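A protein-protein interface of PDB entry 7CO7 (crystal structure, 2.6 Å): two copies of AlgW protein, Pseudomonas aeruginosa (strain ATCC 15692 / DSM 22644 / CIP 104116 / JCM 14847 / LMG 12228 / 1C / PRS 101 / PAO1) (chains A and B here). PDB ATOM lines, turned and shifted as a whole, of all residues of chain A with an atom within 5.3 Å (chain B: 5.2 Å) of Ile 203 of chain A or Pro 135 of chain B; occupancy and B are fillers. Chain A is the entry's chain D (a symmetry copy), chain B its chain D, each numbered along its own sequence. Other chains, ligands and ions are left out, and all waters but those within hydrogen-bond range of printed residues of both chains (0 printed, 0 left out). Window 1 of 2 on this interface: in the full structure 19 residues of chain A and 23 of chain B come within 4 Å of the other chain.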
ATOM      1  N   GLN A 165     -17.415 -10.537 -21.237  1.00  0.00           N
ATOM      2  CA  GLN A 165     -17.714 -11.478 -22.309  1.00  0.00           C
ATOM      3  C   GLN A 165     -18.284 -10.739 -23.514  1.00  0.00           C
ATOM      4  O   GLN A 165     -19.254  -9.996 -23.381  1.00  0.00           O
ATOM      5  CB  GLN A 165     -18.692 -12.546 -21.825  1.00  0.00           C
ATOM      6  CG  GLN A 165     -18.557 -13.871 -22.529  1.00  0.00           C
ATOM      7  CD  GLN A 165     -19.672 -14.806 -22.150  1.00  0.00           C
ATOM      8  OE1 GLN A 165     -19.655 -15.371 -21.063  1.00  0.00           O
ATOM      9  NE2 GLN A 165     -20.659 -14.965 -23.035  1.00  0.00           N
ATOM     10  N   THR A 166     -17.696 -10.960 -24.686  1.00  0.00           N
ATOM     11  CA  THR A 166     -18.141 -10.295 -25.904  1.00  0.00           C
ATOM     12  C   THR A 166     -18.448 -11.296 -27.016  1.00  0.00           C
ATOM     13  O   THR A 166     -17.686 -12.231 -27.250  1.00  0.00           O
ATOM     14  CB  THR A 166     -17.105  -9.275 -26.410  1.00  0.00           C
ATOM     15  OG1 THR A 166     -17.401  -8.973 -27.770  1.00  0.00           O
ATOM     16  CG2 THR A 166     -15.705  -9.841 -26.331  1.00  0.00           C
ATOM     17  N   ALA A 192      -9.118 -14.456 -24.018  1.00  0.00           N
ATOM     18  CA  ALA A 192      -9.446 -15.871 -24.103  1.00  0.00           C
ATOM     19  C   ALA A 192     -10.746 -16.050 -24.859  1.00  0.00           C
ATOM     20  O   ALA A 192     -11.599 -15.162 -24.874  1.00  0.00           O
ATOM     21  CB  ALA A 192      -9.560 -16.492 -22.712  1.00  0.00           C
ATOM     22  N   ILE A 193     -10.888 -17.221 -25.486  1.00  0.00           N
ATOM     23  CA  ILE A 193     -12.157 -17.643 -26.068  1.00  0.00           C
ATOM     24  C   ILE A 193     -12.506 -19.022 -25.538  1.00  0.00           C
ATOM     25  O   ILE A 193     -11.660 -19.747 -25.019  1.00  0.00           O
ATOM     26  CB  ILE A 193     -12.158 -17.661 -27.607  1.00  0.00           C
ATOM     27  CG1 ILE A 193     -11.528 -18.929 -28.166  1.00  0.00           C
ATOM     28  CG2 ILE A 193     -11.394 -16.479 -28.163  1.00  0.00           C
ATOM     29  CD1 ILE A 193     -11.491 -18.881 -29.729  1.00  0.00           C
ATOM     30  N   PHE A 194     -13.789 -19.346 -25.613  1.00  0.00           N
ATOM     31  CA  PHE A 194     -14.288 -20.699 -25.397  1.00  0.00           C
ATOM     32  C   PHE A 194     -14.789 -21.171 -26.740  1.00  0.00           C
ATOM     33  O   PHE A 194     -15.774 -20.643 -27.244  1.00  0.00           O
ATOM     34  CB  PHE A 194     -15.420 -20.768 -24.371  1.00  0.00           C
ATOM     35  CG  PHE A 194     -14.956 -20.848 -22.956  1.00  0.00           C
ATOM     36  CD1 PHE A 194     -13.609 -20.870 -22.658  1.00  0.00           C
ATOM     37  CD2 PHE A 194     -15.869 -20.905 -21.922  1.00  0.00           C
ATOM     38  CE1 PHE A 194     -13.171 -20.943 -21.357  1.00  0.00           C
ATOM     39  CE2 PHE A 194     -15.439 -20.971 -20.614  1.00  0.00           C
ATOM     40  CZ  PHE A 194     -14.084 -20.990 -20.334  1.00  0.00           C
ATOM     41  N   SER A 200     -13.306 -18.372 -33.393  1.00  0.00           N
ATOM     42  CA  SER A 200     -14.399 -17.677 -32.728  1.00  0.00           C
ATOM     43  C   SER A 200     -15.721 -18.398 -32.937  1.00  0.00           C
ATOM     44  O   SER A 200     -16.108 -18.719 -34.064  1.00  0.00           O
ATOM     45  CB  SER A 200     -14.513 -16.233 -33.205  1.00  0.00           C
ATOM     46  OG  SER A 200     -15.685 -15.662 -32.641  1.00  0.00           O
ATOM     47  N   GLN A 201     -16.417 -18.647 -31.835  1.00  0.00           N
ATOM     48  CA  GLN A 201     -17.812 -19.056 -31.880  1.00  0.00           C
ATOM     49  C   GLN A 201     -18.686 -18.063 -31.118  1.00  0.00           C
ATOM     50  O   GLN A 201     -19.796 -18.417 -30.657  1.00  0.00           O
ATOM     51  CB  GLN A 201     -17.945 -20.477 -31.328  1.00  0.00           C
ATOM     52  CG  GLN A 201     -17.571 -21.507 -32.363  1.00  0.00           C
ATOM     53  CD  GLN A 201     -17.313 -22.884 -31.774  1.00  0.00           C
ATOM     54  OE1 GLN A 201     -17.210 -23.065 -30.552  1.00  0.00           O
ATOM     55  NE2 GLN A 201     -17.207 -23.877 -32.658  1.00  0.00           N
ATOM     56  N   GLY A 202     -18.197 -16.836 -30.959  1.00  0.00           N
ATOM     57  CA  GLY A 202     -18.921 -15.824 -30.238  1.00  0.00           C
ATOM     58  C   GLY A 202     -18.852 -15.887 -28.730  1.00  0.00           C
ATOM     59  O   GLY A 202     -19.625 -15.183 -28.083  1.00  0.00           O
ATOM     60  N   ILE A 203     -17.960 -16.677 -28.139  1.00  0.00           N
ATOM     61  CA  ILE A 203     -17.766 -16.632 -26.701  1.00  0.00           C
ATOM     62  C   ILE A 203     -16.343 -16.161 -26.446  1.00  0.00           C
ATOM     63  O   ILE A 203     -15.410 -16.968 -26.454  1.00  0.00           O
ATOM     64  CB  ILE A 203     -18.051 -17.974 -26.028  1.00  0.00           C
ATOM     65  CG1 ILE A 203     -19.339 -18.598 -26.566  1.00  0.00           C
ATOM     66  CG2 ILE A 203     -18.232 -17.750 -24.556  1.00  0.00           C
ATOM     67  CD1 ILE A 203     -20.634 -17.854 -26.109  1.00  0.00           C
ATOM     68  N   GLY A 204     -16.163 -14.861 -26.223  1.00  0.00           N
ATOM     69  CA  GLY A 204     -14.840 -14.291 -26.003  1.00  0.00           C
ATOM     70  C   GLY A 204     -14.782 -13.530 -24.707  1.00  0.00           C
ATOM     71  O   GLY A 204     -15.796 -13.095 -24.173  1.00  0.00           O
ATOM     72  N   PHE A 205     -13.569 -13.389 -24.173  1.00  0.00           N
ATOM     73  CA  PHE A 205     -13.369 -12.793 -22.856  1.00  0.00           C
ATOM     74  C   PHE A 205     -12.240 -11.784 -22.886  1.00  0.00           C
ATOM     75  O   PHE A 205     -11.177 -12.049 -23.433  1.00  0.00           O
ATOM     76  CB  PHE A 205     -13.062 -13.839 -21.816  1.00  0.00           C
ATOM     77  CG  PHE A 205     -14.096 -14.914 -21.727  1.00  0.00           C
ATOM     78  CD1 PHE A 205     -15.298 -14.686 -21.103  1.00  0.00           C
ATOM     79  CD2 PHE A 205     -13.858 -16.157 -22.269  1.00  0.00           C
ATOM     80  CE1 PHE A 205     -16.261 -15.674 -21.020  1.00  0.00           C
ATOM     81  CE2 PHE A 205     -14.808 -17.148 -22.193  1.00  0.00           C
ATOM     82  CZ  PHE A 205     -16.012 -16.903 -21.563  1.00  0.00           C
ATOM     83  N   GLY B 133     -29.309 -17.138 -23.542  1.00  0.00           N
ATOM     84  CA  GLY B 133     -29.264 -18.506 -23.074  1.00  0.00           C
ATOM     85  C   GLY B 133     -27.999 -18.710 -22.282  1.00  0.00           C
ATOM     86  O   GLY B 133     -27.389 -17.749 -21.823  1.00  0.00           O
ATOM     87  N   ASN B 134     -27.581 -19.974 -22.165  1.00  0.00           N
ATOM     88  CA  ASN B 134     -26.457 -20.361 -21.308  1.00  0.00           C
ATOM     89  C   ASN B 134     -25.417 -21.137 -22.110  1.00  0.00           C
ATOM     90  O   ASN B 134     -25.186 -22.329 -21.863  1.00  0.00           O
ATOM     91  CB  ASN B 134     -26.955 -21.193 -20.130  1.00  0.00           C
ATOM     92  CG  ASN B 134     -25.873 -21.497 -19.137  1.00  0.00           C
ATOM     93  OD1 ASN B 134     -24.783 -20.922 -19.185  1.00  0.00           O
ATOM     94  ND2 ASN B 134     -26.163 -22.425 -18.223  1.00  0.00           N
ATOM     95  N   PRO B 135     -24.782 -20.502 -23.093  1.00  0.00           N
ATOM     96  CA  PRO B 135     -23.826 -21.238 -23.924  1.00  0.00           C
ATOM     97  C   PRO B 135     -22.720 -21.863 -23.098  1.00  0.00           C
ATOM     98  O   PRO B 135     -22.087 -21.192 -22.283  1.00  0.00           O
ATOM     99  CB  PRO B 135     -23.273 -20.169 -24.861  1.00  0.00           C
ATOM    100  CG  PRO B 135     -23.678 -18.861 -24.268  1.00  0.00           C
ATOM    101  CD  PRO B 135     -24.981 -19.132 -23.590  1.00  0.00           C
ATOM    102  N   PHE B 136     -22.474 -23.160 -23.344  1.00  0.00           N
ATOM    103  CA  PHE B 136     -21.381 -23.922 -22.735  1.00  0.00           C
ATOM    104  C   PHE B 136     -21.443 -23.912 -21.214  1.00  0.00           C
ATOM    105  O   PHE B 136     -20.449 -24.231 -20.550  1.00  0.00           O
ATOM    106  CB  PHE B 136     -20.020 -23.394 -23.200  1.00  0.00           C
ATOM    107  CG  PHE B 136     -19.822 -23.434 -24.687  1.00  0.00           C
ATOM    108  CD1 PHE B 136     -20.236 -24.514 -25.423  1.00  0.00           C
ATOM    109  CD2 PHE B 136     -19.219 -22.376 -25.340  1.00  0.00           C
ATOM    110  CE1 PHE B 136     -20.042 -24.548 -26.772  1.00  0.00           C
ATOM    111  CE2 PHE B 136     -19.033 -22.395 -26.698  1.00  0.00           C
ATOM    112  CZ  PHE B 136     -19.441 -23.482 -27.412  1.00  0.00           C
ATOM    113  N   GLY B 137     -22.577 -23.513 -20.639  1.00  0.00           N
ATOM    114  CA  GLY B 137     -22.699 -23.403 -19.187  1.00  0.00           C
ATOM    115  C   GLY B 137     -21.909 -22.267 -18.574  1.00  0.00           C
ATOM    116  O   GLY B 137     -21.611 -22.305 -17.377  1.00  0.00           O
ATOM    117  N   VAL B 138     -21.543 -21.261 -19.371  1.00  0.00           N
ATOM    118  CA  VAL B 138     -20.738 -20.151 -18.886  1.00  0.00           C
ATOM    119  C   VAL B 138     -21.522 -19.180 -18.033  1.00  0.00           C
ATOM    120  O   VAL B 138     -20.900 -18.313 -17.391  1.00  0.00           O
ATOM    121  CB  VAL B 138     -20.110 -19.362 -20.040  1.00  0.00           C
ATOM    122  CG1 VAL B 138     -19.036 -18.483 -19.489  1.00  0.00           C
ATOM    123  CG2 VAL B 138     -19.514 -20.319 -21.005  1.00  0.00           C
ATOM    124  N   GLY B 139     -22.846 -19.308 -17.982  1.00  0.00           N
ATOM    125  CA  GLY B 139     -23.720 -18.318 -17.397  1.00  0.00           C
ATOM    126  C   GLY B 139     -24.630 -17.697 -18.442  1.00  0.00           C
ATOM    127  O   GLY B 139     -24.440 -17.858 -19.651  1.00  0.00           O
ATOM    128  N   THR B 141     -25.765 -15.440 -21.070  1.00  0.00           N
ATOM    129  CA  THR B 141     -25.047 -14.542 -21.954  1.00  0.00           C
ATOM    130  C   THR B 141     -25.990 -14.039 -23.035  1.00  0.00           C
ATOM    131  O   THR B 141     -26.890 -14.747 -23.462  1.00  0.00           O
ATOM    132  CB  THR B 141     -23.762 -15.226 -22.552  1.00  0.00           C
ATOM    133  OG1 THR B 141     -23.953 -15.620 -23.906  1.00  0.00           O
ATOM    134  CG2 THR B 141     -23.381 -16.407 -21.754  1.00  0.00           C
ATOM    135  N   ASN B 171     -25.063 -21.353 -29.485  1.00  0.00           N
ATOM    136  CA  ASN B 171     -24.208 -22.470 -29.199  1.00  0.00           C
ATOM    137  C   ASN B 171     -24.935 -23.484 -28.344  1.00  0.00           C
ATOM    138  O   ASN B 171     -26.009 -23.189 -27.776  1.00  0.00           O
ATOM    139  CB  ASN B 171     -22.924 -22.023 -28.470  1.00  0.00           C
ATOM    140  CG  ASN B 171     -21.983 -21.251 -29.356  1.00  0.00           C
ATOM    141  OD1 ASN B 171     -21.395 -21.800 -30.279  1.00  0.00           O
ATOM    142  ND2 ASN B 171     -21.820 -19.973 -29.069  1.00  0.00           N
ATOM    143  N   PRO B 172     -24.408 -24.685 -28.208  1.00  0.00           N
ATOM    144  CA  PRO B 172     -24.933 -25.643 -27.238  1.00  0.00           C
ATOM    145  C   PRO B 172     -25.096 -25.016 -25.857  1.00  0.00           C
ATOM    146  O   PRO B 172     -24.138 -24.508 -25.269  1.00  0.00           O
ATOM    147  CB  PRO B 172     -23.863 -26.733 -27.219  1.00  0.00           C
ATOM    148  CG  PRO B 172     -23.097 -26.577 -28.441  1.00  0.00           C
ATOM    149  CD  PRO B 172     -23.175 -25.163 -28.866  1.00  0.00           C
ATOM    150  N   GLY B 173     -26.310 -25.097 -25.317  1.00  0.00           N
ATOM    151  CA  GLY B 173     -26.644 -24.394 -24.101  1.00  0.00           C
ATOM    152  C   GLY B 173     -27.598 -23.246 -24.309  1.00  0.00           C
ATOM    153  O   GLY B 173     -28.220 -22.792 -23.348  1.00  0.00           O
ATOM    154  N   ASN B 174     -27.735 -22.775 -25.535  1.00  0.00           N
ATOM    155  CA  ASN B 174     -28.730 -21.780 -25.865  1.00  0.00           C
ATOM    156  C   ASN B 174     -30.108 -22.375 -26.124  1.00  0.00           C
ATOM    157  O   ASN B 174     -31.077 -21.618 -26.250  1.00  0.00           O
ATOM    158  CB  ASN B 174     -28.288 -21.005 -27.103  1.00  0.00           C
ATOM    159  CG  ASN B 174     -27.299 -19.899 -26.787  1.00  0.00           C
ATOM    160  OD1 ASN B 174     -26.161 -19.905 -27.275  1.00  0.00           O
ATOM    161  ND2 ASN B 174     -27.733 -18.926 -25.996  1.00  0.00           N
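Printed residues of chain B within 4 Å of Ile 203 of chain A: Pro 135 (3.7 Å), Phe 136 (3.8 Å) and Asn 171 (3.8 Å).
Of chain A, only Ile 203 (3.7 Å) comes within 4 Å of Pro 135 of chain B.
Printed residues of chain A within 4 Å of Phe 136 of chain B: Phe 194 (3.7 Å), Gln 201 (3.9 Å) and Ile 203 (3.8 Å).
Of the printed residues of chain B, Phe 205 of chain A touches Val 138.
Of the printed residues of chain B, Phe 194 of chain A touches Phe 136 and Val 138.
Of the printed residues of chain B, Gln 165 of chain A touches Val 138 and Thr 141.
Of the printed residues of chain A, Thr 141 of chain B touches Gln 165 (3.2 Å).
Gly 204 of chain A touches none of the printed residues of chain B.
The nearest printed residue of chain B that does not touch Ile 203 of chain A is Val 138 of chain B (4.6 Å).
The nearest residue of chain A that does not touch Pro 135 of chain B is Gln 165 of chain A (5.1 Å).
No position is printed for both chains.
Of the 10 pairs that touch across the chains among the printed residues, none has its exchanged pair printed and touching as well.
The backbone NH (N) of Thr 141 of chain B is in hydrogen-bond range of the backbone carbonyl oxygen (O) of Gly 133 of chain B (2.9 Å).
The backbone NH of Val 138 of chain B is in hydrogen-bond range of the side-chain amide oxygen of Asn 134 of chain B (3.3 Å).
O of Pro 172 of chain B is in hydrogen-bond range of N of Phe 136 of chain B, 2.9 Å away.
The backbone NH of Asn 171 of chain B sits at hydrogen-bond distance from the side-chain amide oxygen of Asn 174 of chain B (2.9 Å).
O of Ala 192 of chain A lies within hydrogen-bond range of N of Phe 205 of chain A, at 2.7 Å.
The backbone carbonyl oxygen of Ile 203 of chain A is in hydrogen-bond range of the backbone NH of Phe 194 of chain A (3.0 Å).
OE1 of Gln 165 of chain A touches CG1 of Val 138 of chain B, at 3.5 Å.
Phe 136 of chain B touches Phe 194 of chain A (CE2 to O, 3.7 Å).
Val 138 of chain B touches Phe 194 of chain A.
CZ of Phe 136 of chain B touches OE1 of Gln 201 of chain A, 3.9 Å away.
Ile 203 of chain A touches Pro 135 of chain B.
Ile 203 of chain A touches Phe 136 of chain B.
Asn 171 of chain B touches Ile 203 of chain A.
Val 138 of chain B touches Phe 205 of chain A.
Hydrophobic or aromatic side chains of chain A that line the printed part of chain B: Phe 194, Ile 203 and Phe 205.
Of the 12 printed residues of chain B, 5 touch a printed residue of chain A.
Among the printed residues, 10 pairs touch across the chains.
Among the printed residues, no Asp or Glu carboxylate lies within 4 Å of a Lys or Arg side-chain nitrogen of the other chain.
The side-chain hydroxyl (OG1) of Thr 141 of chain B lies close to the side-chain amide nitrogen (NE2) of Gln 165 of chain A.
ND2 of Asn 171 of chain B sits at hydrogen-bond distance from O of Gln 201 of chain A.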
